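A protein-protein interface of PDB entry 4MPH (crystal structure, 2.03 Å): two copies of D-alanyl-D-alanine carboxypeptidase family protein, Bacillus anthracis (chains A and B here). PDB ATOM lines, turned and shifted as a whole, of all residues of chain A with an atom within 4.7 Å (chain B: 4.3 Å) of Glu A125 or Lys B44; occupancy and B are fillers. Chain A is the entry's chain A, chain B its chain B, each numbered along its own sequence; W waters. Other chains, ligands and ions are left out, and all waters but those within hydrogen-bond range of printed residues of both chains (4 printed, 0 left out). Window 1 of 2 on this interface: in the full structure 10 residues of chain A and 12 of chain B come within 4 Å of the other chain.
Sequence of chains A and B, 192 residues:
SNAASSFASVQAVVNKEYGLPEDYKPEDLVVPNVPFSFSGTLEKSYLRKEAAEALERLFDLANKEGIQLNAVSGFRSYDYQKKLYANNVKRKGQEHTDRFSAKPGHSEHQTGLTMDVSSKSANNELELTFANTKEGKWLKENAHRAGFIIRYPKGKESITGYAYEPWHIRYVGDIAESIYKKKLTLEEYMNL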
ATOM      1  N   SER A 118     -26.288 -18.406 -18.376  1.00  0.00           N
ATOM      2  CA  SER A 118     -25.589 -18.920 -19.543  1.00  0.00           C
ATOM      3  C   SER A 118     -25.247 -20.394 -19.348  1.00  0.00           C
ATOM      4  O   SER A 118     -25.823 -21.068 -18.490  1.00  0.00           O
ATOM      5  CB  SER A 118     -24.341 -18.082 -19.831  1.00  0.00           C
ATOM      6  OG  SER A 118     -23.701 -18.502 -21.039  1.00  0.00           O
ATOM      7  N   ALA A 122     -21.444 -22.099 -23.849  1.00  0.00           N
ATOM      8  CA  ALA A 122     -21.299 -20.717 -24.314  1.00  0.00           C
ATOM      9  C   ALA A 122     -20.251 -19.971 -23.487  1.00  0.00           C
ATOM     10  O   ALA A 122     -20.287 -18.733 -23.398  1.00  0.00           O
ATOM     11  CB  ALA A 122     -22.638 -19.992 -24.241  1.00  0.00           C
ATOM     12  N   ASN A 123     -19.336 -20.726 -22.870  1.00  0.00           N
ATOM     13  CA  ASN A 123     -18.326 -20.161 -21.955  1.00  0.00           C
ATOM     14  C   ASN A 123     -18.866 -19.338 -20.779  1.00  0.00           C
ATOM     15  O   ASN A 123     -18.149 -18.495 -20.222  1.00  0.00           O
ATOM     16  CB  ASN A 123     -17.289 -19.340 -22.729  1.00  0.00           C
ATOM     17  CG  ASN A 123     -16.428 -20.201 -23.616  1.00  0.00           C
ATOM     18  OD1 ASN A 123     -15.655 -21.034 -23.130  1.00  0.00           O
ATOM     19  ND2 ASN A 123     -16.561 -20.020 -24.928  1.00  0.00           N
ATOM     20  N   ASN A 124     -20.118 -19.597 -20.406  1.00  0.00           N
ATOM     21  CA  ASN A 124     -20.815 -18.834 -19.364  1.00  0.00           C
ATOM     22  C   ASN A 124     -20.860 -17.338 -19.636  1.00  0.00           C
ATOM     23  O   ASN A 124     -21.031 -16.529 -18.715  1.00  0.00           O
ATOM     24  CB  ASN A 124     -20.223 -19.116 -17.973  1.00  0.00           C
ATOM     25  CG  ASN A 124     -20.484 -20.548 -17.509  1.00  0.00           C
ATOM     26  OD1 ASN A 124     -21.492 -21.171 -17.888  1.00  0.00           O
ATOM     27  ND2 ASN A 124     -19.566 -21.083 -16.706  1.00  0.00           N
ATOM     28  N   GLU A 125     -20.720 -16.974 -20.906  1.00  0.00           N
ATOM     29  CA  GLU A 125     -20.720 -15.573 -21.303  1.00  0.00           C
ATOM     30  C   GLU A 125     -22.086 -15.124 -21.816  1.00  0.00           C
ATOM     31  O   GLU A 125     -22.893 -15.939 -22.295  1.00  0.00           O
ATOM     32  CB  GLU A 125     -19.598 -15.317 -22.333  1.00  0.00           C
ATOM     33  CG  GLU A 125     -18.213 -15.361 -21.688  1.00  0.00           C
ATOM     34  CD  GLU A 125     -17.070 -15.354 -22.696  1.00  0.00           C
ATOM     35  OE1 GLU A 125     -17.335 -15.245 -23.916  1.00  0.00           O
ATOM     36  OE2 GLU A 125     -15.900 -15.463 -22.262  1.00  0.00           O
ATOM     37  N   LEU A 126     -22.356 -13.827 -21.694  1.00  0.00           N
ATOM     38  CA  LEU A 126     -23.646 -13.273 -22.096  1.00  0.00           C
ATOM     39  C   LEU A 126     -23.498 -12.780 -23.535  1.00  0.00           C
ATOM     40  O   LEU A 126     -23.296 -11.588 -23.792  1.00  0.00           O
ATOM     41  CB  LEU A 126     -24.035 -12.130 -21.154  1.00  0.00           C
ATOM     42  CG  LEU A 126     -23.894 -12.533 -19.684  1.00  0.00           C
ATOM     43  CD1 LEU A 126     -24.337 -11.397 -18.734  1.00  0.00           C
ATOM     44  CD2 LEU A 126     -24.726 -13.798 -19.406  1.00  0.00           C
ATOM     45  N   GLU A 127     -23.544 -13.714 -24.477  1.00  0.00           N
ATOM     46  CA  GLU A 127     -23.346 -13.369 -25.879  1.00  0.00           C
ATOM     47  C   GLU A 127     -24.432 -14.035 -26.707  1.00  0.00           C
ATOM     48  O   GLU A 127     -25.135 -14.928 -26.219  1.00  0.00           O
ATOM     49  CB  GLU A 127     -21.963 -13.825 -26.359  1.00  0.00           C
ATOM     50  CG  GLU A 127     -20.781 -13.169 -25.639  1.00  0.00           C
ATOM     51  CD  GLU A 127     -20.560 -11.717 -26.044  1.00  0.00           C
ATOM     52  OE1 GLU A 127     -21.052 -11.311 -27.121  1.00  0.00           O
ATOM     53  OE2 GLU A 127     -19.886 -10.979 -25.287  1.00  0.00           O
ATOM     54  N   PHE A 130     -25.056 -17.898 -27.120  1.00  0.00           N
ATOM     55  CA  PHE A 130     -25.833 -18.692 -26.173  1.00  0.00           C
ATOM     56  C   PHE A 130     -27.139 -19.181 -26.805  1.00  0.00           C
ATOM     57  O   PHE A 130     -27.617 -20.282 -26.511  1.00  0.00           O
ATOM     58  CB  PHE A 130     -26.112 -17.876 -24.902  1.00  0.00           C
ATOM     59  CG  PHE A 130     -26.972 -18.591 -23.889  1.00  0.00           C
ATOM     60  CD1 PHE A 130     -26.578 -19.816 -23.352  1.00  0.00           C
ATOM     61  CD2 PHE A 130     -28.165 -18.019 -23.444  1.00  0.00           C
ATOM     62  CE1 PHE A 130     -27.371 -20.477 -22.400  1.00  0.00           C
ATOM     63  CE2 PHE A 130     -28.971 -18.668 -22.491  1.00  0.00           C
ATOM     64  CZ  PHE A 130     -28.573 -19.904 -21.965  1.00  0.00           C
ATOM     65  N   PHE B  38     -13.514 -16.019 -12.713  1.00  0.00           N
ATOM     66  CA  PHE B  38     -14.649 -16.848 -13.096  1.00  0.00           C
ATOM     67  C   PHE B  38     -14.375 -18.263 -12.627  1.00  0.00           C
ATOM     68  O   PHE B  38     -13.217 -18.632 -12.415  1.00  0.00           O
ATOM     69  CB  PHE B  38     -14.833 -16.835 -14.625  1.00  0.00           C
ATOM     70  CG  PHE B  38     -13.669 -17.416 -15.378  1.00  0.00           C
ATOM     71  CD1 PHE B  38     -13.646 -18.762 -15.713  1.00  0.00           C
ATOM     72  CD2 PHE B  38     -12.591 -16.613 -15.749  1.00  0.00           C
ATOM     73  CE1 PHE B  38     -12.563 -19.304 -16.408  1.00  0.00           C
ATOM     74  CE2 PHE B  38     -11.501 -17.145 -16.443  1.00  0.00           C
ATOM     75  CZ  PHE B  38     -11.485 -18.493 -16.776  1.00  0.00           C
ATOM     76  N   LEU B  42     -12.426 -23.316 -18.676  1.00  0.00           N
ATOM     77  CA  LEU B  42     -12.941 -22.943 -19.986  1.00  0.00           C
ATOM     78  C   LEU B  42     -11.752 -22.624 -20.874  1.00  0.00           C
ATOM     79  O   LEU B  42     -10.623 -22.576 -20.397  1.00  0.00           O
ATOM     80  CB  LEU B  42     -13.859 -21.726 -19.855  1.00  0.00           C
ATOM     81  CG  LEU B  42     -15.072 -21.887 -18.935  1.00  0.00           C
ATOM     82  CD1 LEU B  42     -15.678 -20.521 -18.622  1.00  0.00           C
ATOM     83  CD2 LEU B  42     -16.112 -22.828 -19.572  1.00  0.00           C
ATOM     84  N   GLU B  43     -11.997 -22.421 -22.163  1.00  0.00           N
ATOM     85  CA  GLU B  43     -10.924 -22.096 -23.105  1.00  0.00           C
ATOM     86  C   GLU B  43     -10.028 -20.959 -22.584  1.00  0.00           C
ATOM     87  O   GLU B  43      -8.798 -21.057 -22.633  1.00  0.00           O
ATOM     88  CB  GLU B  43     -11.549 -21.744 -24.458  1.00  0.00           C
ATOM     89  CG  GLU B  43     -10.608 -21.241 -25.516  1.00  0.00           C
ATOM     90  CD  GLU B  43     -11.311 -21.074 -26.866  1.00  0.00           C
ATOM     91  OE1 GLU B  43     -11.575 -19.911 -27.264  1.00  0.00           O
ATOM     92  OE2 GLU B  43     -11.607 -22.105 -27.526  1.00  0.00           O
ATOM     93  N   LYS B  44     -10.649 -19.915 -22.031  1.00  0.00           N
ATOM     94  CA  LYS B  44      -9.918 -18.749 -21.504  1.00  0.00           C
ATOM     95  C   LYS B  44      -9.153 -19.000 -20.186  1.00  0.00           C
ATOM     96  O   LYS B  44      -8.481 -18.096 -19.669  1.00  0.00           O
ATOM     97  CB  LYS B  44     -10.877 -17.561 -21.327  1.00  0.00           C
ATOM     98  CG  LYS B  44     -11.942 -17.797 -20.256  1.00  0.00           C
ATOM     99  CD  LYS B  44     -12.919 -16.627 -20.152  1.00  0.00           C
ATOM    100  CE  LYS B  44     -14.067 -16.978 -19.181  1.00  0.00           C
ATOM    101  NZ  LYS B  44     -15.030 -15.858 -19.037  1.00  0.00           N
ATOM    102  N   SER B  45      -9.244 -20.219 -19.651  1.00  0.00           N
ATOM    103  CA  SER B  45      -8.459 -20.600 -18.472  1.00  0.00           C
ATOM    104  C   SER B  45      -6.993 -20.866 -18.820  1.00  0.00           C
ATOM    105  O   SER B  45      -6.132 -20.899 -17.934  1.00  0.00           O
ATOM    106  CB  SER B  45      -9.036 -21.868 -17.836  1.00  0.00           C
ATOM    107  OG  SER B  45     -10.376 -21.668 -17.412  1.00  0.00           O
ATOM    108  N   TYR B  46      -6.710 -21.063 -20.104  1.00  0.00           N
ATOM    109  CA  TYR B  46      -5.418 -21.613 -20.513  1.00  0.00           C
ATOM    110  C   TYR B  46      -4.416 -20.581 -21.001  1.00  0.00           C
ATOM    111  O   TYR B  46      -4.798 -19.540 -21.563  1.00  0.00           O
ATOM    112  CB  TYR B  46      -5.607 -22.654 -21.635  1.00  0.00           C
ATOM    113  CG  TYR B  46      -6.320 -23.911 -21.196  1.00  0.00           C
ATOM    114  CD1 TYR B  46      -7.710 -23.969 -21.167  1.00  0.00           C
ATOM    115  CD2 TYR B  46      -5.602 -25.048 -20.822  1.00  0.00           C
ATOM    116  CE1 TYR B  46      -8.373 -25.122 -20.768  1.00  0.00           C
ATOM    117  CE2 TYR B  46      -6.256 -26.214 -20.426  1.00  0.00           C
ATOM    118  CZ  TYR B  46      -7.640 -26.239 -20.399  1.00  0.00           C
ATOM    119  OH  TYR B  46      -8.300 -27.382 -20.004  1.00  0.00           O
ATOM    120  N   VAL B  72      -8.414 -13.045 -15.698  1.00  0.00           N
ATOM    121  CA  VAL B  72      -9.757 -12.866 -16.249  1.00  0.00           C
ATOM    122  C   VAL B  72      -9.977 -13.624 -17.560  1.00  0.00           C
ATOM    123  O   VAL B  72     -11.020 -14.242 -17.751  1.00  0.00           O
ATOM    124  CB  VAL B  72     -10.069 -11.388 -16.453  1.00  0.00           C
ATOM    125  CG1 VAL B  72     -11.476 -11.221 -17.046  1.00  0.00           C
ATOM    126  CG2 VAL B  72      -9.936 -10.640 -15.109  1.00  0.00           C
ATOM    127  N   SER B  73      -9.009 -13.574 -18.471  1.00  0.00           N
ATOM    128  CA  SER B  73      -9.118 -14.369 -19.700  1.00  0.00           C
ATOM    129  C   SER B  73      -7.795 -14.518 -20.447  1.00  0.00           C
ATOM    130  O   SER B  73      -7.133 -13.514 -20.761  1.00  0.00           O
ATOM    131  CB  SER B  73     -10.181 -13.798 -20.644  1.00  0.00           C
ATOM    132  OG  SER B  73     -10.128 -12.382 -20.682  1.00  0.00           O
ATOM    133  N   GLY B  74      -7.430 -15.771 -20.733  1.00  0.00           N
ATOM    134  CA  GLY B  74      -6.198 -16.089 -21.436  1.00  0.00           C
ATOM    135  C   GLY B  74      -6.456 -16.472 -22.887  1.00  0.00           C
ATOM    136  O   GLY B  74      -6.832 -15.631 -23.706  1.00  0.00           O
ATOM    137  N   PHE B  75      -6.243 -17.744 -23.212  1.00  0.00           N
ATOM    138  CA  PHE B  75      -6.392 -18.202 -24.589  1.00  0.00           C
ATOM    139  C   PHE B  75      -7.791 -17.960 -25.157  1.00  0.00           C
ATOM    140  O   PHE B  75      -8.797 -18.224 -24.495  1.00  0.00           O
ATOM    141  CB  PHE B  75      -6.061 -19.689 -24.700  1.00  0.00           C
ATOM    142  CG  PHE B  75      -6.259 -20.240 -26.083  1.00  0.00           C
ATOM    143  CD1 PHE B  75      -5.443 -19.824 -27.129  1.00  0.00           C
ATOM    144  CD2 PHE B  75      -7.264 -21.161 -26.343  1.00  0.00           C
ATOM    145  CE1 PHE B  75      -5.614 -20.326 -28.426  1.00  0.00           C
ATOM    146  CE2 PHE B  75      -7.447 -21.667 -27.634  1.00  0.00           C
ATOM    147  CZ  PHE B  75      -6.616 -21.247 -28.675  1.00  0.00           C
ATOM    148  N   ARG B  76      -7.843 -17.428 -26.377  1.00  0.00           N
ATOM    149  CA  ARG B  76      -9.093 -17.321 -27.125  1.00  0.00           C
ATOM    150  C   ARG B  76      -8.833 -17.845 -28.535  1.00  0.00           C
ATOM    151  O   ARG B  76      -7.992 -17.317 -29.248  1.00  0.00           O
ATOM    152  CB  ARG B  76      -9.574 -15.866 -27.204  1.00  0.00           C
ATOM    153  CG  ARG B  76      -9.872 -15.175 -25.855  1.00  0.00           C
ATOM    154  CD  ARG B  76     -11.137 -15.707 -25.174  1.00  0.00           C
ATOM    155  NE  ARG B  76     -11.652 -14.762 -24.173  1.00  0.00           N
ATOM    156  CZ  ARG B  76     -12.833 -14.864 -23.563  1.00  0.00           C
ATOM    157  NH1 ARG B  76     -13.649 -15.878 -23.836  1.00  0.00           N
ATOM    158  NH2 ARG B  76     -13.202 -13.945 -22.675  1.00  0.00           N
ATOM    159  N   TYR B  80     -13.550 -18.744 -31.682  1.00  0.00           N
ATOM    160  CA  TYR B  80     -14.223 -17.904 -30.698  1.00  0.00           C
ATOM    161  C   TYR B  80     -14.196 -16.457 -31.167  1.00  0.00           C
ATOM    162  O   TYR B  80     -15.220 -15.779 -31.170  1.00  0.00           O
ATOM    163  CB  TYR B  80     -13.557 -18.020 -29.329  1.00  0.00           C
ATOM    164  CG  TYR B  80     -14.107 -17.046 -28.312  1.00  0.00           C
ATOM    165  CD1 TYR B  80     -15.205 -17.380 -27.526  1.00  0.00           C
ATOM    166  CD2 TYR B  80     -13.532 -15.794 -28.136  1.00  0.00           C
ATOM    167  CE1 TYR B  80     -15.715 -16.490 -26.587  1.00  0.00           C
ATOM    168  CE2 TYR B  80     -14.036 -14.897 -27.195  1.00  0.00           C
ATOM    169  CZ  TYR B  80     -15.126 -15.248 -26.431  1.00  0.00           C
ATOM    170  OH  TYR B  80     -15.615 -14.354 -25.503  1.00  0.00           O
HETATM  171  O   HOH W   1     -13.483 -19.280 -22.835  1.00  0.00           O
HETATM  172  O   HOH W   2     -14.429 -23.107 -23.436  1.00  0.00           O
HETATM  173  O   HOH W   3     -14.850 -20.973 -27.145  1.00  0.00           O
HETATM  174  O   HOH W   4     -17.111 -17.312 -17.644  1.00  0.00           O
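The side-chain carboxylate (OE2) of Glu A125 is in salt-bridge range of the side-chain amino group (NZ) of Lys B44.
The side-chain carboxylate (OE2) of Glu A125 lies within salt-bridge range of the guanidinium group (NH1) of Arg B76 (2.8 Å).
OH of Tyr B80 lies within hydrogen-bond range of OE1 of Glu A125, at 2.5 Å.
The side-chain hydroxyl (OG) of Ser A118 sits at hydrogen-bond distance from the backbone carbonyl oxygen (O) of Glu A125 (3.0 Å).
N of Leu B42 sits at hydrogen-bond distance from OG of Ser B45, at 2.9 Å.
O of Lys B44 is in hydrogen-bond range of N of Gly B74, 2.8 Å away.
The side-chain hydroxyl (OH) of Tyr B80 lies within hydrogen-bond range of the guanidinium group (NH1) of Arg B76.
Among the printed residues, pairs that only touch across the chains: Asn A123 with Leu B42 (3.6 Å) and Asn A123 with Tyr B80 (3.9 Å).
Lys B44 touches one residue of chain A.
Of the printed residues of chain A, Tyr B80 touches Asn A123 and Glu A125.
Of the printed residues of chain B, Asn A123 touches Leu B42 and Tyr B80.
The nearest printed residue of chain B that does not touch Glu A125 is Ser B73 (6.2 Å).
The nearest residue of chain A that does not touch Lys B44 is Asn A123 (4.3 Å).
The nearest printed residue of chain A that does not touch Tyr B80 is Glu A127 (5.3 Å).
Printed residues of chain A that touch a printed residue of chain B: Asn A123 and Glu A125.
Among the printed residues, 5 pairs touch across the chains.
Among the printed residues, Asp or Glu carboxylates within 4 Å of a Lys or Arg side-chain nitrogen of the other chain: Glu A125 with Lys B44 (3.4 Å) and Glu A125 with Arg B76 (2.8 Å).
No position is printed for both chains.
Of the 5 pairs that touch across the chains among the printed residues, none has its exchanged pair printed and touching as well.
Water W2 lies within hydrogen-bond range of OD1 of Asn A123 and N of Glu B43.
Water W1 lies within hydrogen-bond range of the side-chain amide oxygen (OD1) of Asn A123 (2.8 Å) and the backbone NH (N) of Lys B44 (3.0 Å).
Water W4 lies within hydrogen-bond range of the side-chain amino group of Lys B44 (2.9 Å) and the backbone carbonyl oxygen of Asn A123 (3.0 Å).
Water W3 lies within hydrogen-bond range of ND2 of Asn A123 (3.0 Å) and OE1 of Glu B43 (3.4 Å).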
